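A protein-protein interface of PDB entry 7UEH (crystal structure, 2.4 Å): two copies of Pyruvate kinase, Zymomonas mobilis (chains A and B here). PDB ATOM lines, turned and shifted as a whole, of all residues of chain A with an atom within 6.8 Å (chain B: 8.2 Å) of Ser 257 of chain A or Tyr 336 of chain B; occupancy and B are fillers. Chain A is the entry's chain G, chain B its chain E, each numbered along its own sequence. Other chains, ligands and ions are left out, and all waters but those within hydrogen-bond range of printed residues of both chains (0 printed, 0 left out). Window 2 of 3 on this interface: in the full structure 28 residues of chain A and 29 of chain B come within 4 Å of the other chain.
NE of Arg 332 of chain B is in salt-bridge range of OE2 of Glu 256 of chain A (2.6 Å).
The backbone carbonyl oxygen of Leu 254 of chain A lies within hydrogen-bond range of the side-chain hydroxyl of Ser 257 of chain A (2.8 Å).
The backbone carbonyl oxygen of Ser 257 of chain A sits at hydrogen-bond distance from the side-chain hydroxyl of Thr 261 of chain A (3.2 Å).
Among the printed residues, merely in contact across the chains: Pro 255 of chain A with Val 297 of chain B (3.6 Å), Pro 255 of chain A with Arg 332 of chain B (3.9 Å), Glu 256 of chain A with Ile 333 of chain B (3.8 Å), Glu 256 of chain A with Tyr 336 of chain B (3.7 Å), Ser 257 of chain A with Tyr 336 of chain B (3.3 Å), Pro 259 of chain A with Val 297 of chain B (3.7 Å), Pro 259 of chain A with Ala 301 of chain B (3.5 Å), Pro 260 of chain A with Tyr 305 of chain B (3.3 Å) and Pro 260 of chain A with Ala 340 of chain B (3.8 Å).
Printed residues of chain B within 4 Å of Pro 255 of chain A: Val 297 and Arg 332.
Printed residues of chain B within 4 Å of Glu 256 of chain A: Arg 332, Ile 333 and Tyr 336.
Ser 257 of chain A touches just one residue of chain B: Tyr 336.
Printed residues of chain B within 4 Å of Pro 259 of chain A: Val 297 and Ala 301.
Of the printed residues of chain A, Tyr 305 of chain B touches Pro 260.
Of the printed residues of chain A, Arg 332 of chain B touches Pro 255 (3.9 Å) and Glu 256 (2.6 Å).
Tyr 336 of chain B touches two residues of chain A.
The nearest residue of chain B that does not touch Ser 257 of chain A is Val 297 of chain B (5.7 Å).
The nearest residue of chain A that does not touch Tyr 336 of chain B is Pro 260 of chain A (4.1 Å).
The nearest printed residue of chain B that does not touch Pro 255 of chain A is Met 329 of chain B (4.3 Å).
Printed residues of chain A that touch a printed residue of chain B: Pro 255, Glu 256, Ser 257, Pro 259 and Pro 260.
Hydrophobic or aromatic side chains of chain A that line the printed part of chain B: Pro 255, Pro 259 and Pro 260.
Along chain B the printed residues that touch a printed residue of chain A span positions 297 to 340.
Among the printed residues, 10 pairs touch across the chains.
No position is printed for both chains.
Of the 10 pairs that touch across the chains among the printed residues, none has its exchanged pair printed and touching as well.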
ATOM      1  N   LEU A 249     -13.463  -0.399  -2.984  1.00  0.00           N
ATOM      2  CA  LEU A 249     -13.371  -0.932  -1.633  1.00  0.00           C
ATOM      3  C   LEU A 249     -14.039  -2.288  -1.541  1.00  0.00           C
ATOM      4  O   LEU A 249     -13.523  -3.198  -0.891  1.00  0.00           O
ATOM      5  CB  LEU A 249     -14.046   0.004  -0.645  1.00  0.00           C
ATOM      6  CG  LEU A 249     -13.196   0.997   0.109  1.00  0.00           C
ATOM      7  CD1 LEU A 249     -14.150   1.771   1.008  1.00  0.00           C
ATOM      8  CD2 LEU A 249     -12.111   0.313   0.879  1.00  0.00           C
ATOM      9  N   GLY A 250     -15.215  -2.419  -2.148  1.00  0.00           N
ATOM     10  CA  GLY A 250     -15.942  -3.673  -2.129  1.00  0.00           C
ATOM     11  C   GLY A 250     -15.353  -4.778  -2.997  1.00  0.00           C
ATOM     12  O   GLY A 250     -15.780  -5.929  -2.871  1.00  0.00           O
ATOM     13  N   CYS A 253     -11.926  -5.330  -0.544  1.00  0.00           N
ATOM     14  CA  CYS A 253     -12.358  -5.966   0.698  1.00  0.00           C
ATOM     15  C   CYS A 253     -13.675  -6.691   0.436  1.00  0.00           C
ATOM     16  O   CYS A 253     -14.274  -6.612  -0.658  1.00  0.00           O
ATOM     17  CB  CYS A 253     -12.527  -4.960   1.856  1.00  0.00           C
ATOM     18  SG  CYS A 253     -11.392  -3.509   1.934  1.00  0.00           S
ATOM     19  N   LEU A 254     -14.135  -7.405   1.445  1.00  0.00           N
ATOM     20  CA  LEU A 254     -15.445  -8.017   1.339  1.00  0.00           C
ATOM     21  C   LEU A 254     -16.500  -6.931   1.094  1.00  0.00           C
ATOM     22  O   LEU A 254     -16.464  -5.871   1.747  1.00  0.00           O
ATOM     23  CB  LEU A 254     -15.740  -8.815   2.600  1.00  0.00           C
ATOM     24  CG  LEU A 254     -14.924 -10.107   2.748  1.00  0.00           C
ATOM     25  CD1 LEU A 254     -15.385 -10.845   3.996  1.00  0.00           C
ATOM     26  CD2 LEU A 254     -15.081 -11.028   1.555  1.00  0.00           C
ATOM     27  N   PRO A 255     -17.427  -7.127   0.147  1.00  0.00           N
ATOM     28  CA  PRO A 255     -18.492  -6.127  -0.011  1.00  0.00           C
ATOM     29  C   PRO A 255     -19.296  -5.951   1.260  1.00  0.00           C
ATOM     30  O   PRO A 255     -19.668  -4.813   1.571  1.00  0.00           O
ATOM     31  CB  PRO A 255     -19.324  -6.663  -1.182  1.00  0.00           C
ATOM     32  CG  PRO A 255     -19.004  -8.133  -1.248  1.00  0.00           C
ATOM     33  CD  PRO A 255     -17.588  -8.266  -0.776  1.00  0.00           C
ATOM     34  N   GLU A 256     -19.510  -7.018   2.047  1.00  0.00           N
ATOM     35  CA  GLU A 256     -20.225  -6.866   3.319  1.00  0.00           C
ATOM     36  C   GLU A 256     -19.438  -6.085   4.353  1.00  0.00           C
ATOM     37  O   GLU A 256     -20.021  -5.679   5.369  1.00  0.00           O
ATOM     38  CB  GLU A 256     -20.615  -8.214   3.932  1.00  0.00           C
ATOM     39  CG  GLU A 256     -19.490  -9.216   4.256  1.00  0.00           C
ATOM     40  CD  GLU A 256     -19.169 -10.151   3.070  1.00  0.00           C
ATOM     41  OE1 GLU A 256     -18.764  -9.628   2.021  1.00  0.00           O
ATOM     42  OE2 GLU A 256     -19.342 -11.387   3.167  1.00  0.00           O
ATOM     43  N   SER A 257     -18.154  -5.815   4.116  1.00  0.00           N
ATOM     44  CA  SER A 257     -17.390  -5.012   5.066  1.00  0.00           C
ATOM     45  C   SER A 257     -17.370  -3.527   4.741  1.00  0.00           C
ATOM     46  O   SER A 257     -16.825  -2.758   5.524  1.00  0.00           O
ATOM     47  CB  SER A 257     -15.937  -5.481   5.135  1.00  0.00           C
ATOM     48  OG  SER A 257     -15.179  -4.905   4.072  1.00  0.00           O
ATOM     49  N   VAL A 258     -17.894  -3.111   3.597  1.00  0.00           N
ATOM     50  CA  VAL A 258     -17.902  -1.696   3.267  1.00  0.00           C
ATOM     51  C   VAL A 258     -18.715  -0.885   4.268  1.00  0.00           C
ATOM     52  O   VAL A 258     -18.246   0.193   4.671  1.00  0.00           O
ATOM     53  CB  VAL A 258     -18.405  -1.485   1.817  1.00  0.00           C
ATOM     54  CG1 VAL A 258     -18.450   0.002   1.485  1.00  0.00           C
ATOM     55  CG2 VAL A 258     -17.481  -2.217   0.835  1.00  0.00           C
ATOM     56  N   PRO A 259     -19.903  -1.305   4.682  1.00  0.00           N
ATOM     57  CA  PRO A 259     -20.777  -0.387   5.466  1.00  0.00           C
ATOM     58  C   PRO A 259     -20.144  -0.002   6.792  1.00  0.00           C
ATOM     59  O   PRO A 259     -20.119   1.188   7.116  1.00  0.00           O
ATOM     60  CB  PRO A 259     -22.066  -1.194   5.661  1.00  0.00           C
ATOM     61  CG  PRO A 259     -22.071  -2.145   4.502  1.00  0.00           C
ATOM     62  CD  PRO A 259     -20.624  -2.511   4.259  1.00  0.00           C
ATOM     63  N   PRO A 260     -19.584  -0.949   7.572  1.00  0.00           N
ATOM     64  CA  PRO A 260     -18.854  -0.539   8.793  1.00  0.00           C
ATOM     65  C   PRO A 260     -17.651   0.312   8.494  1.00  0.00           C
ATOM     66  O   PRO A 260     -17.335   1.212   9.246  1.00  0.00           O
ATOM     67  CB  PRO A 260     -18.429  -1.866   9.427  1.00  0.00           C
ATOM     68  CG  PRO A 260     -19.338  -2.860   8.854  1.00  0.00           C
ATOM     69  CD  PRO A 260     -19.630  -2.407   7.453  1.00  0.00           C
ATOM     70  N   THR A 261     -16.995   0.091   7.381  1.00  0.00           N
ATOM     71  CA  THR A 261     -15.863   0.938   7.026  1.00  0.00           C
ATOM     72  C   THR A 261     -16.323   2.325   6.564  1.00  0.00           C
ATOM     73  O   THR A 261     -15.607   3.303   6.792  1.00  0.00           O
ATOM     74  CB  THR A 261     -15.012   0.196   5.982  1.00  0.00           C
ATOM     75  OG1 THR A 261     -14.413  -0.956   6.618  1.00  0.00           O
ATOM     76  CG2 THR A 261     -13.939   1.095   5.415  1.00  0.00           C
ATOM     77  N   GLN A 262     -17.517   2.426   5.950  1.00  0.00           N
ATOM     78  CA  GLN A 262     -18.103   3.722   5.640  1.00  0.00           C
ATOM     79  C   GLN A 262     -18.498   4.472   6.917  1.00  0.00           C
ATOM     80  O   GLN A 262     -18.248   5.679   7.033  1.00  0.00           O
ATOM     81  CB  GLN A 262     -19.307   3.529   4.714  1.00  0.00           C
ATOM     82  CG  GLN A 262     -20.028   4.814   4.336  1.00  0.00           C
ATOM     83  CD  GLN A 262     -21.244   4.622   3.417  1.00  0.00           C
ATOM     84  OE1 GLN A 262     -21.265   3.811   2.461  1.00  0.00           O
ATOM     85  NE2 GLN A 262     -22.241   5.406   3.677  1.00  0.00           N
ATOM     86  N   GLY B   9     -24.589 -17.263  14.054  1.00  0.00           N
ATOM     87  CA  GLY B   9     -23.535 -16.285  14.130  1.00  0.00           C
ATOM     88  C   GLY B   9     -23.993 -14.862  13.910  1.00  0.00           C
ATOM     89  O   GLY B   9     -23.146 -13.956  13.812  1.00  0.00           O
ATOM     90  N   ARG B  10     -25.305 -14.646  13.819  1.00  0.00           N
ATOM     91  CA  ARG B  10     -25.907 -13.325  13.787  1.00  0.00           C
ATOM     92  C   ARG B  10     -27.342 -13.471  14.282  1.00  0.00           C
ATOM     93  O   ARG B  10     -27.913 -14.575  14.290  1.00  0.00           O
ATOM     94  CB  ARG B  10     -25.822 -12.715  12.382  1.00  0.00           C
ATOM     95  CG  ARG B  10     -26.019 -13.709  11.237  1.00  0.00           C
ATOM     96  CD  ARG B  10     -27.510 -13.994  10.934  1.00  0.00           C
ATOM     97  NE  ARG B  10     -27.696 -14.863   9.762  1.00  0.00           N
ATOM     98  CZ  ARG B  10     -28.872 -15.355   9.353  1.00  0.00           C
ATOM     99  NH1 ARG B  10     -29.998 -15.080  10.003  1.00  0.00           N
ATOM    100  NH2 ARG B  10     -28.926 -16.146   8.284  1.00  0.00           N
ATOM    101  N   VAL B 297     -25.952  -3.358  -0.426  1.00  0.00           N
ATOM    102  CA  VAL B 297     -25.375  -3.879   0.807  1.00  0.00           C
ATOM    103  C   VAL B 297     -25.559  -2.862   1.943  1.00  0.00           C
ATOM    104  O   VAL B 297     -25.852  -3.229   3.083  1.00  0.00           O
ATOM    105  CB  VAL B 297     -23.911  -4.264   0.575  1.00  0.00           C
ATOM    106  CG1 VAL B 297     -23.226  -4.577   1.901  1.00  0.00           C
ATOM    107  CG2 VAL B 297     -23.884  -5.464  -0.333  1.00  0.00           C
ATOM    108  N   ALA B 301     -27.263  -3.434   5.693  1.00  0.00           N
ATOM    109  CA  ALA B 301     -26.537  -3.074   6.912  1.00  0.00           C
ATOM    110  C   ALA B 301     -27.288  -2.007   7.709  1.00  0.00           C
ATOM    111  O   ALA B 301     -27.384  -2.114   8.923  1.00  0.00           O
ATOM    112  CB  ALA B 301     -25.128  -2.582   6.589  1.00  0.00           C
ATOM    113  N   ILE B 304     -29.947  -3.390   9.721  1.00  0.00           N
ATOM    114  CA  ILE B 304     -29.457  -4.104  10.891  1.00  0.00           C
ATOM    115  C   ILE B 304     -29.127  -3.121  12.015  1.00  0.00           C
ATOM    116  O   ILE B 304     -29.522  -3.331  13.175  1.00  0.00           O
ATOM    117  CB  ILE B 304     -28.252  -4.974  10.497  1.00  0.00           C
ATOM    118  CG1 ILE B 304     -28.740  -6.103   9.578  1.00  0.00           C
ATOM    119  CG2 ILE B 304     -27.549  -5.491  11.740  1.00  0.00           C
ATOM    120  CD1 ILE B 304     -27.640  -6.944   8.947  1.00  0.00           C
ATOM    121  N   TYR B 305     -28.398  -2.039  11.675  1.00  0.00           N
ATOM    122  CA  TYR B 305     -28.010  -0.989  12.611  1.00  0.00           C
ATOM    123  C   TYR B 305     -29.215  -0.309  13.261  1.00  0.00           C
ATOM    124  O   TYR B 305     -29.114   0.162  14.389  1.00  0.00           O
ATOM    125  CB  TYR B 305     -27.173   0.087  11.910  1.00  0.00           C
ATOM    126  CG  TYR B 305     -25.770  -0.291  11.527  1.00  0.00           C
ATOM    127  CD1 TYR B 305     -24.880  -0.832  12.458  1.00  0.00           C
ATOM    128  CD2 TYR B 305     -25.312  -0.077  10.243  1.00  0.00           C
ATOM    129  CE1 TYR B 305     -23.586  -1.173  12.096  1.00  0.00           C
ATOM    130  CE2 TYR B 305     -24.020  -0.422   9.875  1.00  0.00           C
ATOM    131  CZ  TYR B 305     -23.159  -0.980  10.800  1.00  0.00           C
ATOM    132  OH  TYR B 305     -21.857  -1.310  10.425  1.00  0.00           O
ATOM    133  N   MET B 329     -25.953 -13.812   0.610  1.00  0.00           N
ATOM    134  CA  MET B 329     -25.424 -12.472   0.814  1.00  0.00           C
ATOM    135  C   MET B 329     -26.091 -11.822   2.027  1.00  0.00           C
ATOM    136  O   MET B 329     -25.418 -11.157   2.821  1.00  0.00           O
ATOM    137  CB  MET B 329     -25.599 -11.651  -0.476  1.00  0.00           C
ATOM    138  CG  MET B 329     -25.130 -10.185  -0.423  1.00  0.00           C
ATOM    139  SD  MET B 329     -23.422 -10.091   0.142  1.00  0.00           S
ATOM    140  CE  MET B 329     -22.572 -10.576  -1.349  1.00  0.00           C
ATOM    141  N   MET B 330     -27.417 -12.022   2.202  1.00  0.00           N
ATOM    142  CA  MET B 330     -28.098 -11.542   3.413  1.00  0.00           C
ATOM    143  C   MET B 330     -27.418 -12.069   4.673  1.00  0.00           C
ATOM    144  O   MET B 330     -27.242 -11.336   5.658  1.00  0.00           O
ATOM    145  CB  MET B 330     -29.570 -11.973   3.436  1.00  0.00           C
ATOM    146  CG  MET B 330     -30.443 -11.405   2.303  1.00  0.00           C
ATOM    147  SD  MET B 330     -30.560  -9.603   2.297  1.00  0.00           S
ATOM    148  CE  MET B 330     -32.224  -9.397   2.924  1.00  0.00           C
ATOM    149  N   HIS B 331     -27.071 -13.355   4.678  1.00  0.00           N
ATOM    150  CA  HIS B 331     -26.454 -13.925   5.855  1.00  0.00           C
ATOM    151  C   HIS B 331     -25.063 -13.377   6.024  1.00  0.00           C
ATOM    152  O   HIS B 331     -24.621 -13.151   7.144  1.00  0.00           O
ATOM    153  CB  HIS B 331     -26.398 -15.442   5.752  1.00  0.00           C
ATOM    154  CG  HIS B 331     -25.453 -16.069   6.727  1.00  0.00           C
ATOM    155  ND1 HIS B 331     -25.756 -16.221   8.061  1.00  0.00           N
ATOM    156  CD2 HIS B 331     -24.202 -16.562   6.567  1.00  0.00           C
ATOM    157  CE1 HIS B 331     -24.746 -16.808   8.677  1.00  0.00           C
ATOM    158  NE2 HIS B 331     -23.792 -17.027   7.792  1.00  0.00           N
ATOM    159  N   ARG B 332     -24.349 -13.185   4.913  1.00  0.00           N
ATOM    160  CA  ARG B 332     -22.981 -12.681   4.992  1.00  0.00           C
ATOM    161  C   ARG B 332     -22.942 -11.232   5.485  1.00  0.00           C
ATOM    162  O   ARG B 332     -22.024 -10.851   6.221  1.00  0.00           O
ATOM    163  CB  ARG B 332     -22.295 -12.776   3.631  1.00  0.00           C
ATOM    164  CG  ARG B 332     -21.696 -14.089   3.325  1.00  0.00           C
ATOM    165  CD  ARG B 332     -21.310 -14.142   1.856  1.00  0.00           C
ATOM    166  NE  ARG B 332     -20.380 -13.091   1.437  1.00  0.00           N
ATOM    167  CZ  ARG B 332     -20.057 -12.844   0.161  1.00  0.00           C
ATOM    168  NH1 ARG B 332     -20.580 -13.563  -0.838  1.00  0.00           N
ATOM    169  NH2 ARG B 332     -19.215 -11.868  -0.123  1.00  0.00           N
ATOM    170  N   ILE B 333     -23.913 -10.407   5.084  1.00  0.00           N
ATOM    171  CA  ILE B 333     -23.925  -9.016   5.522  1.00  0.00           C
ATOM    172  C   ILE B 333     -24.169  -8.933   7.024  1.00  0.00           C
ATOM    173  O   ILE B 333     -23.463  -8.212   7.746  1.00  0.00           O
ATOM    174  CB  ILE B 333     -24.972  -8.213   4.740  1.00  0.00           C
ATOM    175  CG1 ILE B 333     -24.506  -8.106   3.299  1.00  0.00           C
ATOM    176  CG2 ILE B 333     -25.178  -6.836   5.363  1.00  0.00           C
ATOM    177  CD1 ILE B 333     -25.588  -7.701   2.318  1.00  0.00           C
ATOM    178  N   ALA B 334     -25.145  -9.694   7.526  1.00  0.00           N
ATOM    179  CA  ALA B 334     -25.403  -9.678   8.970  1.00  0.00           C
ATOM    180  C   ALA B 334     -24.241 -10.287   9.769  1.00  0.00           C
ATOM    181  O   ALA B 334     -23.862  -9.772  10.835  1.00  0.00           O
ATOM    182  CB  ALA B 334     -26.713 -10.413   9.276  1.00  0.00           C
ATOM    183  N   SER B 335     -23.705 -11.416   9.320  1.00  0.00           N
ATOM    184  CA  SER B 335     -22.571 -11.990  10.033  1.00  0.00           C
ATOM    185  C   SER B 335     -21.502 -10.932  10.244  1.00  0.00           C
ATOM    186  O   SER B 335     -20.974 -10.784  11.347  1.00  0.00           O
ATOM    187  CB  SER B 335     -21.976 -13.175   9.276  1.00  0.00           C
ATOM    188  OG  SER B 335     -22.844 -14.268   9.341  1.00  0.00           O
ATOM    189  N   TYR B 336     -21.177 -10.178   9.188  1.00  0.00           N
ATOM    190  CA  TYR B 336     -20.078  -9.221   9.289  1.00  0.00           C
ATOM    191  C   TYR B 336     -20.483  -7.991  10.095  1.00  0.00           C
ATOM    192  O   TYR B 336     -19.796  -7.604  11.036  1.00  0.00           O
ATOM    193  CB  TYR B 336     -19.610  -8.802   7.898  1.00  0.00           C
ATOM    194  CG  TYR B 336     -18.280  -8.130   7.946  1.00  0.00           C
ATOM    195  CD1 TYR B 336     -18.158  -6.824   8.407  1.00  0.00           C
ATOM    196  CD2 TYR B 336     -17.138  -8.807   7.574  1.00  0.00           C
ATOM    197  CE1 TYR B 336     -16.936  -6.214   8.510  1.00  0.00           C
ATOM    198  CE2 TYR B 336     -15.901  -8.202   7.672  1.00  0.00           C
ATOM    199  CZ  TYR B 336     -15.815  -6.899   8.137  1.00  0.00           C
ATOM    200  OH  TYR B 336     -14.593  -6.275   8.207  1.00  0.00           O
ATOM    201  N   VAL B 337     -21.618  -7.383   9.760  1.00  0.00           N
ATOM    202  CA  VAL B 337     -21.996  -6.119  10.391  1.00  0.00           C
ATOM    203  C   VAL B 337     -22.211  -6.313  11.884  1.00  0.00           C
ATOM    204  O   VAL B 337     -21.704  -5.547  12.711  1.00  0.00           O
ATOM    205  CB  VAL B 337     -23.232  -5.532   9.688  1.00  0.00           C
ATOM    206  CG1 VAL B 337     -23.869  -4.416  10.502  1.00  0.00           C
ATOM    207  CG2 VAL B 337     -22.851  -5.057   8.195  1.00  0.00           C
ATOM    208  N   GLU B 338     -22.921  -7.361  12.267  1.00  0.00           N
ATOM    209  CA  GLU B 338     -23.206  -7.521  13.693  1.00  0.00           C
ATOM    210  C   GLU B 338     -21.946  -7.734  14.505  1.00  0.00           C
ATOM    211  O   GLU B 338     -21.927  -7.407  15.687  1.00  0.00           O
ATOM    212  CB  GLU B 338     -24.150  -8.686  13.949  1.00  0.00           C
ATOM    213  CG  GLU B 338     -25.521  -8.410  13.458  1.00  0.00           C
ATOM    214  CD  GLU B 338     -26.530  -9.441  13.867  1.00  0.00           C
ATOM    215  OE1 GLU B 338     -26.194 -10.323  14.696  1.00  0.00           O
ATOM    216  OE2 GLU B 338     -27.660  -9.359  13.337  1.00  0.00           O
ATOM    217  N   ASN B 339     -20.902  -8.294  13.901  1.00  0.00           N
ATOM    218  CA  ASN B 339     -19.661  -8.574  14.607  1.00  0.00           C
ATOM    219  C   ASN B 339     -18.544  -7.599  14.253  1.00  0.00           C
ATOM    220  O   ASN B 339     -17.399  -7.826  14.652  1.00  0.00           O
ATOM    221  CB  ASN B 339     -19.203 -10.002  14.336  1.00  0.00           C
ATOM    222  CG  ASN B 339     -20.180 -11.043  14.853  1.00  0.00           C
ATOM    223  OD1 ASN B 339     -20.186 -11.375  16.031  1.00  0.00           O
ATOM    224  ND2 ASN B 339     -21.024 -11.557  13.965  1.00  0.00           N
ATOM    225  N   ALA B 340     -18.849  -6.504  13.493  1.00  0.00           N
ATOM    226  CA  ALA B 340     -17.895  -5.432  13.205  1.00  0.00           C
ATOM    227  C   ALA B 340     -18.064  -4.282  14.203  1.00  0.00           C
ATOM    228  O   ALA B 340     -19.089  -4.184  14.878  1.00  0.00           O
ATOM    229  CB  ALA B 340     -18.106  -4.931  11.769  1.00  0.00           C
ATOM    230  N   PRO B 341     -17.100  -3.382  14.340  1.00  0.00           N
ATOM    231  CA  PRO B 341     -17.292  -2.268  15.282  1.00  0.00           C
ATOM    232  C   PRO B 341     -18.400  -1.336  14.842  1.00  0.00           C
ATOM    233  O   PRO B 341     -18.682  -1.185  13.651  1.00  0.00           O
ATOM    234  CB  PRO B 341     -15.948  -1.537  15.271  1.00  0.00           C
ATOM    235  CG  PRO B 341     -14.987  -2.611  14.975  1.00  0.00           C
ATOM    236  CD  PRO B 341     -15.699  -3.471  13.912  1.00  0.00           C
ATOM    237  N   TYR B 343     -21.639  -1.611  15.821  1.00  0.00           N
ATOM    238  CA  TYR B 343     -22.963  -2.199  15.737  1.00  0.00           C
ATOM    239  C   TYR B 343     -23.821  -1.875  16.954  1.00  0.00           C
ATOM    240  O   TYR B 343     -24.877  -1.252  16.812  1.00  0.00           O
ATOM    241  CB  TYR B 343     -22.836  -3.700  15.567  1.00  0.00           C
ATOM    242  CG  TYR B 343     -24.086  -4.434  15.828  1.00  0.00           C
ATOM    243  CD1 TYR B 343     -25.141  -4.392  14.922  1.00  0.00           C
ATOM    244  CD2 TYR B 343     -24.233  -5.167  16.978  1.00  0.00           C
ATOM    245  CE1 TYR B 343     -26.295  -5.083  15.153  1.00  0.00           C
ATOM    246  CE2 TYR B 343     -25.378  -5.840  17.218  1.00  0.00           C
ATOM    247  CZ  TYR B 343     -26.403  -5.814  16.277  1.00  0.00           C
ATOM    248  OH  TYR B 343     -27.551  -6.490  16.488  1.00  0.00           O
